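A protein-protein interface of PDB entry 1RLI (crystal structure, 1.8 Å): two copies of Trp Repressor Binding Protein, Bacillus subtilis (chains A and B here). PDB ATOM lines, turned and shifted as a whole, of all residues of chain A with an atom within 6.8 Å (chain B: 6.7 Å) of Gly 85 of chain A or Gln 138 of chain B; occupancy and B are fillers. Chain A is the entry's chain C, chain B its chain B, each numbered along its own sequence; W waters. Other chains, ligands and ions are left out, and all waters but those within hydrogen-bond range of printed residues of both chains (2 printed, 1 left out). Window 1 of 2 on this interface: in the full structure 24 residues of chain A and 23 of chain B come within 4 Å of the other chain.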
ATOM      1  N   THR A  79       2.230 -15.322 -17.346  1.00  0.00           N
ATOM      2  CA  THR A  79       2.859 -14.085 -16.960  1.00  0.00           C
ATOM      3  C   THR A  79       2.831 -12.973 -17.987  1.00  0.00           C
ATOM      4  O   THR A  79       2.842 -13.209 -19.186  1.00  0.00           O
ATOM      5  CB  THR A  79       4.346 -14.347 -16.599  1.00  0.00           C
ATOM      6  OG1 THR A  79       4.953 -13.134 -16.160  1.00  0.00           O
ATOM      7  CG2 THR A  79       5.122 -14.859 -17.810  1.00  0.00           C
ATOM      8  N   PRO A  80       2.716 -11.730 -17.517  1.00  0.00           N
ATOM      9  CA  PRO A  80       2.732 -10.613 -18.449  1.00  0.00           C
ATOM     10  C   PRO A  80       4.223 -10.494 -18.818  1.00  0.00           C
ATOM     11  O   PRO A  80       5.083 -10.996 -18.078  1.00  0.00           O
ATOM     12  CB  PRO A  80       2.258  -9.432 -17.585  1.00  0.00           C
ATOM     13  CG  PRO A  80       2.634  -9.831 -16.189  1.00  0.00           C
ATOM     14  CD  PRO A  80       2.265 -11.302 -16.179  1.00  0.00           C
ATOM     15  N   ILE A  81       4.530  -9.886 -19.958  1.00  0.00           N
ATOM     16  CA  ILE A  81       5.925  -9.693 -20.344  1.00  0.00           C
ATOM     17  C   ILE A  81       6.328  -8.276 -19.916  1.00  0.00           C
ATOM     18  O   ILE A  81       5.847  -7.288 -20.469  1.00  0.00           O
ATOM     19  CB  ILE A  81       6.111  -9.869 -21.866  1.00  0.00           C
ATOM     20  CG1 ILE A  81       5.755 -11.309 -22.257  1.00  0.00           C
ATOM     21  CG2 ILE A  81       7.535  -9.565 -22.267  1.00  0.00           C
ATOM     22  CD1 ILE A  81       5.811 -11.577 -23.751  1.00  0.00           C
ATOM     23  N   TYR A  82       7.174  -8.190 -18.896  1.00  0.00           N
ATOM     24  CA  TYR A  82       7.661  -6.896 -18.390  1.00  0.00           C
ATOM     25  C   TYR A  82       9.123  -6.762 -18.761  1.00  0.00           C
ATOM     26  O   TYR A  82       9.937  -7.589 -18.352  1.00  0.00           O
ATOM     27  CB  TYR A  82       7.597  -6.805 -16.861  1.00  0.00           C
ATOM     28  CG  TYR A  82       6.221  -6.775 -16.240  1.00  0.00           C
ATOM     29  CD1 TYR A  82       5.112  -6.331 -16.955  1.00  0.00           C
ATOM     30  CD2 TYR A  82       6.041  -7.162 -14.914  1.00  0.00           C
ATOM     31  CE1 TYR A  82       3.846  -6.273 -16.353  1.00  0.00           C
ATOM     32  CE2 TYR A  82       4.792  -7.109 -14.309  1.00  0.00           C
ATOM     33  CZ  TYR A  82       3.703  -6.666 -15.032  1.00  0.00           C
ATOM     34  OH  TYR A  82       2.463  -6.630 -14.426  1.00  0.00           O
ATOM     35  N   TRP A  83       9.461  -5.710 -19.502  1.00  0.00           N
ATOM     36  CA  TRP A  83      10.847  -5.482 -19.900  1.00  0.00           C
ATOM     37  C   TRP A  83      11.463  -6.730 -20.550  1.00  0.00           C
ATOM     38  O   TRP A  83      12.585  -7.146 -20.227  1.00  0.00           O
ATOM     39  CB  TRP A  83      11.653  -5.024 -18.685  1.00  0.00           C
ATOM     40  CG  TRP A  83      11.200  -3.679 -18.218  1.00  0.00           C
ATOM     41  CD1 TRP A  83      10.247  -3.403 -17.273  1.00  0.00           C
ATOM     42  CD2 TRP A  83      11.598  -2.424 -18.771  1.00  0.00           C
ATOM     43  NE1 TRP A  83      10.027  -2.041 -17.212  1.00  0.00           N
ATOM     44  CE2 TRP A  83      10.843  -1.419 -18.121  1.00  0.00           C
ATOM     45  CE3 TRP A  83      12.521  -2.051 -19.760  1.00  0.00           C
ATOM     46  CZ2 TRP A  83      10.983  -0.062 -18.428  1.00  0.00           C
ATOM     47  CZ3 TRP A  83      12.668  -0.701 -20.069  1.00  0.00           C
ATOM     48  CH2 TRP A  83      11.896   0.280 -19.402  1.00  0.00           C
ATOM     49  N   PHE A  84      10.684  -7.327 -21.447  1.00  0.00           N
ATOM     50  CA  PHE A  84      11.096  -8.500 -22.218  1.00  0.00           C
ATOM     51  C   PHE A  84      11.380  -9.751 -21.392  1.00  0.00           C
ATOM     52  O   PHE A  84      11.988 -10.723 -21.866  1.00  0.00           O
ATOM     53  CB  PHE A  84      12.284  -8.083 -23.098  1.00  0.00           C
ATOM     54  CG  PHE A  84      11.979  -6.859 -23.922  1.00  0.00           C
ATOM     55  CD1 PHE A  84      11.148  -6.948 -25.036  1.00  0.00           C
ATOM     56  CD2 PHE A  84      12.430  -5.598 -23.513  1.00  0.00           C
ATOM     57  CE1 PHE A  84      10.750  -5.788 -25.738  1.00  0.00           C
ATOM     58  CE2 PHE A  84      12.041  -4.445 -24.197  1.00  0.00           C
ATOM     59  CZ  PHE A  84      11.206  -4.536 -25.303  1.00  0.00           C
ATOM     60  N   GLY A  85      10.881  -9.744 -20.162  1.00  0.00           N
ATOM     61  CA  GLY A  85      11.070 -10.891 -19.291  1.00  0.00           C
ATOM     62  C   GLY A  85       9.757 -11.245 -18.618  1.00  0.00           C
ATOM     63  O   GLY A  85       8.704 -10.752 -19.000  1.00  0.00           O
ATOM     64  N   MET A  86       9.813 -12.122 -17.623  1.00  0.00           N
ATOM     65  CA  MET A  86       8.591 -12.502 -16.913  1.00  0.00           C
ATOM     66  C   MET A  86       8.300 -11.433 -15.866  1.00  0.00           C
ATOM     67  O   MET A  86       9.024 -10.448 -15.770  1.00  0.00           O
ATOM     68  CB  MET A  86       8.779 -13.875 -16.251  1.00  0.00           C
ATOM     69  CG  MET A  86       9.923 -13.949 -15.250  1.00  0.00           C
ATOM     70  SD  MET A  86      10.155 -15.656 -14.636  1.00  0.00           S
ATOM     71  CE  MET A  86      11.189 -16.386 -15.969  1.00  0.00           C
ATOM     72  N   SER A  87       7.233 -11.599 -15.096  1.00  0.00           N
ATOM     73  CA  SER A  87       6.929 -10.609 -14.064  1.00  0.00           C
ATOM     74  C   SER A  87       7.915 -10.694 -12.889  1.00  0.00           C
ATOM     75  O   SER A  87       8.620 -11.688 -12.725  1.00  0.00           O
ATOM     76  CB  SER A  87       5.507 -10.816 -13.542  1.00  0.00           C
ATOM     77  OG  SER A  87       5.419 -11.982 -12.747  1.00  0.00           O
ATOM     78  N   ALA A 122       2.291 -16.104 -22.028  1.00  0.00           N
ATOM     79  CA  ALA A 122       2.904 -14.791 -21.803  1.00  0.00           C
ATOM     80  C   ALA A 122       2.269 -13.733 -22.694  1.00  0.00           C
ATOM     81  O   ALA A 122       2.068 -13.944 -23.895  1.00  0.00           O
ATOM     82  CB  ALA A 122       4.420 -14.851 -22.054  1.00  0.00           C
ATOM     83  N   LYS A 131       9.576 -10.304 -29.919  1.00  0.00           N
ATOM     84  CA  LYS A 131      10.352  -9.835 -28.772  1.00  0.00           C
ATOM     85  C   LYS A 131      10.211 -10.666 -27.510  1.00  0.00           C
ATOM     86  O   LYS A 131      10.969 -10.479 -26.556  1.00  0.00           O
ATOM     87  CB  LYS A 131      10.010  -8.371 -28.490  1.00  0.00           C
ATOM     88  CG  LYS A 131      10.497  -7.457 -29.613  1.00  0.00           C
ATOM     89  CD  LYS A 131      10.061  -6.017 -29.428  1.00  0.00           C
ATOM     90  CE  LYS A 131      10.419  -5.183 -30.658  1.00  0.00           C
ATOM     91  NZ  LYS A 131       9.982  -3.754 -30.538  1.00  0.00           N
ATOM     92  N   PRO A 134      13.059 -14.488 -26.559  1.00  0.00           N
ATOM     93  CA  PRO A 134      14.128 -14.792 -25.606  1.00  0.00           C
ATOM     94  C   PRO A 134      13.554 -15.340 -24.310  1.00  0.00           C
ATOM     95  O   PRO A 134      14.123 -16.241 -23.702  1.00  0.00           O
ATOM     96  CB  PRO A 134      14.804 -13.446 -25.409  1.00  0.00           C
ATOM     97  CG  PRO A 134      14.722 -12.841 -26.817  1.00  0.00           C
ATOM     98  CD  PRO A 134      13.281 -13.184 -27.216  1.00  0.00           C
ATOM     99  N   LEU A 135      12.423 -14.778 -23.872  1.00  0.00           N
ATOM    100  CA  LEU A 135      11.796 -15.236 -22.647  1.00  0.00           C
ATOM    101  C   LEU A 135      11.370 -16.704 -22.785  1.00  0.00           C
ATOM    102  O   LEU A 135      11.562 -17.512 -21.876  1.00  0.00           O
ATOM    103  CB  LEU A 135      10.572 -14.349 -22.316  1.00  0.00           C
ATOM    104  CG  LEU A 135       9.710 -14.867 -21.153  1.00  0.00           C
ATOM    105  CD1 LEU A 135      10.570 -14.988 -19.893  1.00  0.00           C
ATOM    106  CD2 LEU A 135       8.536 -13.906 -20.910  1.00  0.00           C
ATOM    107  N   ILE A 136      10.774 -17.054 -23.919  1.00  0.00           N
ATOM    108  CA  ILE A 136      10.364 -18.441 -24.114  1.00  0.00           C
ATOM    109  C   ILE A 136      11.609 -19.343 -24.088  1.00  0.00           C
ATOM    110  O   ILE A 136      11.573 -20.453 -23.548  1.00  0.00           O
ATOM    111  CB  ILE A 136       9.582 -18.602 -25.445  1.00  0.00           C
ATOM    112  CG1 ILE A 136       8.270 -17.791 -25.375  1.00  0.00           C
ATOM    113  CG2 ILE A 136       9.233 -20.074 -25.691  1.00  0.00           C
ATOM    114  CD1 ILE A 136       7.393 -18.128 -24.170  1.00  0.00           C
ATOM    115  N   GLN A 138      14.362 -18.701 -22.429  1.00  0.00           N
ATOM    116  CA  GLN A 138      14.831 -18.746 -21.055  1.00  0.00           C
ATOM    117  C   GLN A 138      14.003 -19.832 -20.338  1.00  0.00           C
ATOM    118  O   GLN A 138      14.535 -20.678 -19.597  1.00  0.00           O
ATOM    119  CB  GLN A 138      14.611 -17.366 -20.411  1.00  0.00           C
ATOM    120  CG  GLN A 138      15.206 -17.204 -19.029  1.00  0.00           C
ATOM    121  CD  GLN A 138      14.976 -15.798 -18.489  1.00  0.00           C
ATOM    122  OE1 GLN A 138      13.892 -15.478 -17.997  1.00  0.00           O
ATOM    123  NE2 GLN A 138      15.990 -14.947 -18.609  1.00  0.00           N
ATOM    124  N   PHE A 139      12.689 -19.823 -20.552  1.00  0.00           N
ATOM    125  CA  PHE A 139      11.834 -20.856 -19.954  1.00  0.00           C
ATOM    126  C   PHE A 139      12.283 -22.254 -20.415  1.00  0.00           C
ATOM    127  O   PHE A 139      12.291 -23.196 -19.627  1.00  0.00           O
ATOM    128  CB  PHE A 139      10.374 -20.636 -20.346  1.00  0.00           C
ATOM    129  CG  PHE A 139       9.631 -19.712 -19.419  1.00  0.00           C
ATOM    130  CD1 PHE A 139       9.517 -20.024 -18.067  1.00  0.00           C
ATOM    131  CD2 PHE A 139       9.033 -18.554 -19.899  1.00  0.00           C
ATOM    132  CE1 PHE A 139       8.817 -19.202 -17.194  1.00  0.00           C
ATOM    133  CE2 PHE A 139       8.332 -17.719 -19.053  1.00  0.00           C
ATOM    134  CZ  PHE A 139       8.220 -18.044 -17.678  1.00  0.00           C
ATOM    135  N   PHE B  84      19.073 -18.796 -15.717  1.00  0.00           N
ATOM    136  CA  PHE B  84      19.254 -18.335 -17.090  1.00  0.00           C
ATOM    137  C   PHE B  84      18.796 -16.905 -17.345  1.00  0.00           C
ATOM    138  O   PHE B  84      18.526 -16.514 -18.475  1.00  0.00           O
ATOM    139  CB  PHE B  84      18.555 -19.335 -18.013  1.00  0.00           C
ATOM    140  CG  PHE B  84      18.937 -20.761 -17.709  1.00  0.00           C
ATOM    141  CD1 PHE B  84      20.158 -21.278 -18.162  1.00  0.00           C
ATOM    142  CD2 PHE B  84      18.131 -21.556 -16.892  1.00  0.00           C
ATOM    143  CE1 PHE B  84      20.582 -22.557 -17.801  1.00  0.00           C
ATOM    144  CE2 PHE B  84      18.544 -22.842 -16.529  1.00  0.00           C
ATOM    145  CZ  PHE B  84      19.768 -23.341 -16.981  1.00  0.00           C
ATOM    146  N   GLY B  85      18.757 -16.123 -16.276  1.00  0.00           N
ATOM    147  CA  GLY B  85      18.369 -14.733 -16.388  1.00  0.00           C
ATOM    148  C   GLY B  85      19.176 -13.920 -15.397  1.00  0.00           C
ATOM    149  O   GLY B  85      20.189 -14.373 -14.863  1.00  0.00           O
ATOM    150  N   MET B  86      18.732 -12.706 -15.131  1.00  0.00           N
ATOM    151  CA  MET B  86      19.463 -11.871 -14.199  1.00  0.00           C
ATOM    152  C   MET B  86      19.069 -12.177 -12.766  1.00  0.00           C
ATOM    153  O   MET B  86      18.259 -13.074 -12.503  1.00  0.00           O
ATOM    154  CB  MET B  86      19.196 -10.410 -14.499  1.00  0.00           C
ATOM    155  CG  MET B  86      17.726 -10.086 -14.599  1.00  0.00           C
ATOM    156  SD  MET B  86      17.505  -8.304 -14.879  1.00  0.00           S
ATOM    157  CE  MET B  86      17.939  -8.120 -16.616  1.00  0.00           C
ATOM    158  N   LYS B  91      16.300  -7.519 -11.594  1.00  0.00           N
ATOM    159  CA  LYS B  91      15.003  -7.552 -12.262  1.00  0.00           C
ATOM    160  C   LYS B  91      14.038  -6.537 -11.615  1.00  0.00           C
ATOM    161  O   LYS B  91      13.331  -5.788 -12.331  1.00  0.00           O
ATOM    162  CB  LYS B  91      14.423  -8.976 -12.179  1.00  0.00           C
ATOM    163  CG  LYS B  91      12.955  -9.065 -12.572  1.00  0.00           C
ATOM    164  CD  LYS B  91      12.713  -8.507 -13.978  1.00  0.00           C
ATOM    165  CE  LYS B  91      11.419  -9.066 -14.550  1.00  0.00           C
ATOM    166  NZ  LYS B  91      11.077  -8.431 -15.843  1.00  0.00           N
ATOM    167  N   LEU B 133      22.641 -16.893 -23.512  1.00  0.00           N
ATOM    168  CA  LEU B 133      22.356 -16.051 -24.681  1.00  0.00           C
ATOM    169  C   LEU B 133      20.954 -15.431 -24.678  1.00  0.00           C
ATOM    170  O   LEU B 133      20.779 -14.289 -25.114  1.00  0.00           O
ATOM    171  CB  LEU B 133      22.653 -16.814 -25.979  1.00  0.00           C
ATOM    172  CG  LEU B 133      24.172 -17.124 -26.094  1.00  0.00           C
ATOM    173  CD1 LEU B 133      24.436 -17.806 -27.423  1.00  0.00           C
ATOM    174  CD2 LEU B 133      25.025 -15.857 -25.949  1.00  0.00           C
ATOM    175  N   PRO B 134      19.930 -16.165 -24.206  1.00  0.00           N
ATOM    176  CA  PRO B 134      18.607 -15.527 -24.193  1.00  0.00           C
ATOM    177  C   PRO B 134      18.648 -14.282 -23.294  1.00  0.00           C
ATOM    178  O   PRO B 134      18.044 -13.255 -23.607  1.00  0.00           O
ATOM    179  CB  PRO B 134      17.698 -16.625 -23.644  1.00  0.00           C
ATOM    180  CG  PRO B 134      18.318 -17.860 -24.283  1.00  0.00           C
ATOM    181  CD  PRO B 134      19.811 -17.630 -24.065  1.00  0.00           C
ATOM    182  N   LEU B 135      19.367 -14.360 -22.176  1.00  0.00           N
ATOM    183  CA  LEU B 135      19.467 -13.191 -21.290  1.00  0.00           C
ATOM    184  C   LEU B 135      20.121 -12.007 -22.025  1.00  0.00           C
ATOM    185  O   LEU B 135      19.722 -10.821 -21.857  1.00  0.00           O
ATOM    186  CB  LEU B 135      20.286 -13.552 -20.035  1.00  0.00           C
ATOM    187  CG  LEU B 135      20.733 -12.404 -19.123  1.00  0.00           C
ATOM    188  CD1 LEU B 135      19.508 -11.689 -18.559  1.00  0.00           C
ATOM    189  CD2 LEU B 135      21.580 -12.957 -17.991  1.00  0.00           C
ATOM    190  N   ILE B 136      21.123 -12.305 -22.845  1.00  0.00           N
ATOM    191  CA  ILE B 136      21.786 -11.253 -23.596  1.00  0.00           C
ATOM    192  C   ILE B 136      20.781 -10.643 -24.582  1.00  0.00           C
ATOM    193  O   ILE B 136      20.754  -9.428 -24.774  1.00  0.00           O
ATOM    194  CB  ILE B 136      23.037 -11.797 -24.350  1.00  0.00           C
ATOM    195  CG1 ILE B 136      24.093 -12.218 -23.318  1.00  0.00           C
ATOM    196  CG2 ILE B 136      23.651 -10.699 -25.286  1.00  0.00           C
ATOM    197  CD1 ILE B 136      24.546 -11.070 -22.397  1.00  0.00           C
ATOM    198  N   GLN B 137      19.947 -11.479 -25.192  1.00  0.00           N
ATOM    199  CA  GLN B 137      18.938 -10.971 -26.128  1.00  0.00           C
ATOM    200  C   GLN B 137      17.900 -10.110 -25.385  1.00  0.00           C
ATOM    201  O   GLN B 137      17.405  -9.121 -25.925  1.00  0.00           O
ATOM    202  CB  GLN B 137      18.272 -12.144 -26.870  1.00  0.00           C
ATOM    203  CG  GLN B 137      19.214 -12.792 -27.873  1.00  0.00           C
ATOM    204  CD  GLN B 137      18.594 -14.000 -28.556  1.00  0.00           C
ATOM    205  OE1 GLN B 137      18.769 -14.204 -29.760  1.00  0.00           O
ATOM    206  NE2 GLN B 137      17.873 -14.815 -27.787  1.00  0.00           N
ATOM    207  N   GLN B 138      17.560 -10.485 -24.154  1.00  0.00           N
ATOM    208  CA  GLN B 138      16.603  -9.690 -23.384  1.00  0.00           C
ATOM    209  C   GLN B 138      17.217  -8.316 -23.115  1.00  0.00           C
ATOM    210  O   GLN B 138      16.546  -7.292 -23.243  1.00  0.00           O
ATOM    211  CB  GLN B 138      16.262 -10.361 -22.050  1.00  0.00           C
ATOM    212  CG  GLN B 138      15.442 -11.636 -22.166  1.00  0.00           C
ATOM    213  CD  GLN B 138      15.128 -12.225 -20.808  1.00  0.00           C
ATOM    214  OE1 GLN B 138      16.013 -12.360 -19.957  1.00  0.00           O
ATOM    215  NE2 GLN B 138      13.864 -12.580 -20.594  1.00  0.00           N
ATOM    216  N   PHE B 139      18.489  -8.289 -22.729  1.00  0.00           N
ATOM    217  CA  PHE B 139      19.153  -7.000 -22.475  1.00  0.00           C
ATOM    218  C   PHE B 139      19.162  -6.167 -23.754  1.00  0.00           C
ATOM    219  O   PHE B 139      18.944  -4.959 -23.713  1.00  0.00           O
ATOM    220  CB  PHE B 139      20.591  -7.209 -22.006  1.00  0.00           C
ATOM    221  CG  PHE B 139      20.732  -7.334 -20.518  1.00  0.00           C
ATOM    222  CD1 PHE B 139      20.366  -6.285 -19.689  1.00  0.00           C
ATOM    223  CD2 PHE B 139      21.278  -8.491 -19.947  1.00  0.00           C
ATOM    224  CE1 PHE B 139      20.539  -6.369 -18.289  1.00  0.00           C
ATOM    225  CE2 PHE B 139      21.456  -8.596 -18.560  1.00  0.00           C
ATOM    226  CZ  PHE B 139      21.086  -7.532 -17.725  1.00  0.00           C
ATOM    227  N   GLU B 140      19.423  -6.812 -24.891  1.00  0.00           N
ATOM    228  CA  GLU B 140      19.418  -6.110 -26.171  1.00  0.00           C
ATOM    229  C   GLU B 140      18.053  -5.434 -26.369  1.00  0.00           C
ATOM    230  O   GLU B 140      17.995  -4.285 -26.802  1.00  0.00           O
ATOM    231  CB  GLU B 140      19.701  -7.092 -27.318  1.00  0.00           C
ATOM    232  CG  GLU B 140      20.125  -6.433 -28.625  1.00  0.00           C
ATOM    233  CD  GLU B 140      18.974  -5.833 -29.383  1.00  0.00           C
ATOM    234  OE1 GLU B 140      17.872  -6.419 -29.315  1.00  0.00           O
ATOM    235  OE2 GLU B 140      19.176  -4.795 -30.062  1.00  0.00           O
ATOM    236  N   HIS B 141      16.959  -6.136 -26.060  1.00  0.00           N
ATOM    237  CA  HIS B 141      15.625  -5.540 -26.217  1.00  0.00           C
ATOM    238  C   HIS B 141      15.381  -4.394 -25.226  1.00  0.00           C
ATOM    239  O   HIS B 141      14.788  -3.375 -25.595  1.00  0.00           O
ATOM    240  CB  HIS B 141      14.528  -6.600 -26.065  1.00  0.00           C
ATOM    241  CG  HIS B 141      14.456  -7.559 -27.213  1.00  0.00           C
ATOM    242  ND1 HIS B 141      14.567  -7.159 -28.530  1.00  0.00           N
ATOM    243  CD2 HIS B 141      14.265  -8.900 -27.244  1.00  0.00           C
ATOM    244  CE1 HIS B 141      14.453  -8.213 -29.320  1.00  0.00           C
ATOM    245  NE2 HIS B 141      14.270  -9.282 -28.564  1.00  0.00           N
ATOM    246  N   ILE B 142      15.820  -4.571 -23.978  1.00  0.00           N
ATOM    247  CA  ILE B 142      15.668  -3.540 -22.948  1.00  0.00           C
ATOM    248  C   ILE B 142      16.420  -2.291 -23.377  1.00  0.00           C
ATOM    249  O   ILE B 142      15.878  -1.178 -23.355  1.00  0.00           O
ATOM    250  CB  ILE B 142      16.246  -4.019 -21.598  1.00  0.00           C
ATOM    251  CG1 ILE B 142      15.423  -5.199 -21.098  1.00  0.00           C
ATOM    252  CG2 ILE B 142      16.203  -2.917 -20.548  1.00  0.00           C
ATOM    253  CD1 ILE B 142      16.034  -5.888 -19.883  1.00  0.00           C
ATOM    254  N   PHE B 143      17.670  -2.461 -23.785  1.00  0.00           N
ATOM    255  CA  PHE B 143      18.449  -1.291 -24.181  1.00  0.00           C
ATOM    256  C   PHE B 143      17.900  -0.599 -25.422  1.00  0.00           C
ATOM    257  O   PHE B 143      17.864   0.637 -25.492  1.00  0.00           O
ATOM    258  CB  PHE B 143      19.903  -1.691 -24.403  1.00  0.00           C
ATOM    259  CG  PHE B 143      20.572  -2.219 -23.170  1.00  0.00           C
ATOM    260  CD1 PHE B 143      20.268  -1.695 -21.914  1.00  0.00           C
ATOM    261  CD2 PHE B 143      21.526  -3.223 -23.261  1.00  0.00           C
ATOM    262  CE1 PHE B 143      20.904  -2.165 -20.772  1.00  0.00           C
ATOM    263  CE2 PHE B 143      22.168  -3.697 -22.123  1.00  0.00           C
ATOM    264  CZ  PHE B 143      21.856  -3.169 -20.877  1.00  0.00           C
ATOM    265  N   PHE B 150      23.939  -0.812 -27.023  1.00  0.00           N
ATOM    266  CA  PHE B 150      24.434  -2.012 -26.308  1.00  0.00           C
ATOM    267  C   PHE B 150      25.817  -2.263 -26.905  1.00  0.00           C
ATOM    268  O   PHE B 150      25.943  -2.966 -27.910  1.00  0.00           O
ATOM    269  CB  PHE B 150      23.491  -3.202 -26.586  1.00  0.00           C
ATOM    270  CG  PHE B 150      23.780  -4.450 -25.763  1.00  0.00           C
ATOM    271  CD1 PHE B 150      24.714  -4.440 -24.733  1.00  0.00           C
ATOM    272  CD2 PHE B 150      23.038  -5.619 -25.978  1.00  0.00           C
ATOM    273  CE1 PHE B 150      24.906  -5.574 -23.914  1.00  0.00           C
ATOM    274  CE2 PHE B 150      23.211  -6.759 -25.163  1.00  0.00           C
ATOM    275  CZ  PHE B 150      24.142  -6.739 -24.133  1.00  0.00           C
HETATM  276  O   HOH W   1      12.612 -13.268 -17.426  1.00  0.00           O
HETATM  277  O   HOH W   2      12.997  -8.455 -17.558  1.00  0.00           O
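The side-chain sulfur (SD) of Met 86 of chain B lies within hydrogen-bond range of the backbone NH (N) of Lys 91 of chain B, at 3.6 Å. A ring nitrogen (ND1) of His 141 of chain B lies within hydrogen-bond range of the side-chain carboxylate (OE1) of Glu 140 of chain B (3.5 Å).
Water W2 lies within hydrogen-bond range of NZ of Lys 91 of chain B (2.6 Å), O of Trp 83 of chain A (3.0 Å) and O of Tyr 82 of chain A (3.3 Å). Water W1 lies within hydrogen-bond range of OE1 of Gln 138 of chain A (2.6 Å), N of Met 86 of chain A (3.0 Å) and NE2 of Gln 138 of chain B (3.5 Å).
Of the 16 printed residues of chain B, 8 touch a printed residue of chain A. Printed residues of chain B that touch a printed residue of chain A: Phe 84, Gly 85, Lys 91, Pro 134, Gln 137, Gln 138, His 141 and Ile 142. Hydrophobic or aromatic side chains of chain B within 4 Å of the printed part of chain A: Pro 134, His 141 and Ile 142. Along chain B the printed residues that touch a printed residue of chain A span positions 84 to 142. Among the printed residues, no Asp or Glu carboxylate lies within 4 Å of a Lys or Arg side-chain nitrogen of the other chain.
Of the printed residues of chain B, Gly 85 of chain A touches Gln 138. Of the printed residues of chain A, Gly 85 of chain B touches Gln 138 (3.3 Å). Of the printed residues of chain A, Gln 138 of chain B touches Phe 84 (2.9 Å), Gly 85 (3.5 Å), Pro 134 (3.8 Å), Leu 135 (3.9 Å) and Gln 138 (2.9 Å). Of the printed residues of chain A, Ile 142 of chain B touches Trp 83 and Phe 84. The nearest printed residue of chain A that does not touch Gln 138 of chain B is Trp 83 of chain A (5.0 Å).
Phe 84 of chain A touches Gln 138 of chain B, and with the chains exchanged Gln 138 of chain A touches Phe 84 of chain B. Gly 85 of chain A touches Gln 138 of chain B, and with the chains exchanged Gln 138 of chain A touches Gly 85 of chain B. Pro 134 of chain A touches Gln 138 of chain B, but with the chains exchanged Gln 138 of chain A does not touch Pro 134 of chain B (4.1 Å). Gln 138 of chain B touches its own counterpart, Gln 138 of chain A. Positions printed for both chains: 84, 85, 86, 134, 135, 136, 138 and 139. Of the 16 pairs that touch across the chains among the printed residues, 6 have their exchanged pair printed and touching as well.
The backbone carbonyl oxygen of Phe 84 of chain B lies within hydrogen-bond range of the side-chain amide nitrogen of Gln 138 of chain A, 3.0 Å away. The side-chain amino group of Lys 91 of chain B is in hydrogen-bond range of the backbone carbonyl oxygen of Tyr 82 of chain A. The side-chain amino group (NZ) of Lys 91 of chain B lies within hydrogen-bond range of the backbone carbonyl oxygen (O) of Met 86 of chain A (2.9 Å). The backbone carbonyl oxygen of Phe 84 of chain A is in hydrogen-bond range of the side-chain amide nitrogen of Gln 138 of chain B (2.9 Å). The side-chain amide oxygen (OE1) of Gln 138 of chain B is in hydrogen-bond range of the side-chain amide nitrogen (NE2) of Gln 138 of chain A, at 2.9 Å.
Trp 83 of chain A touches Ile 142 of chain B (O to CG1, 3.6 Å). Phe 84 of chain A touches His 141 of chain B (CE2 to O, 3.3 Å). CA of Gly 85 of chain A touches NE2 of Gln 138 of chain B, at 3.5 Å. CD2 of His 141 of chain B touches O of Lys 131 of chain A (3.7 Å). CB of Pro 134 of chain B touches O of Pro 134 of chain A, 3.6 Å away. Gln 137 of chain B touches Pro 134 of chain A (CB to CG, 3.6 Å). Pro 134 of chain A touches Gln 138 of chain B (CB to CG, 3.8 Å). Pro 134 of chain A touches His 141 of chain B (CG to CD2, 3.99 Å). Leu 135 of chain A touches Gln 138 of chain B (CA to NE2, 3.9 Å). Gln 138 of chain A touches Gly 85 of chain B (NE2 to CA, 3.3 Å).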
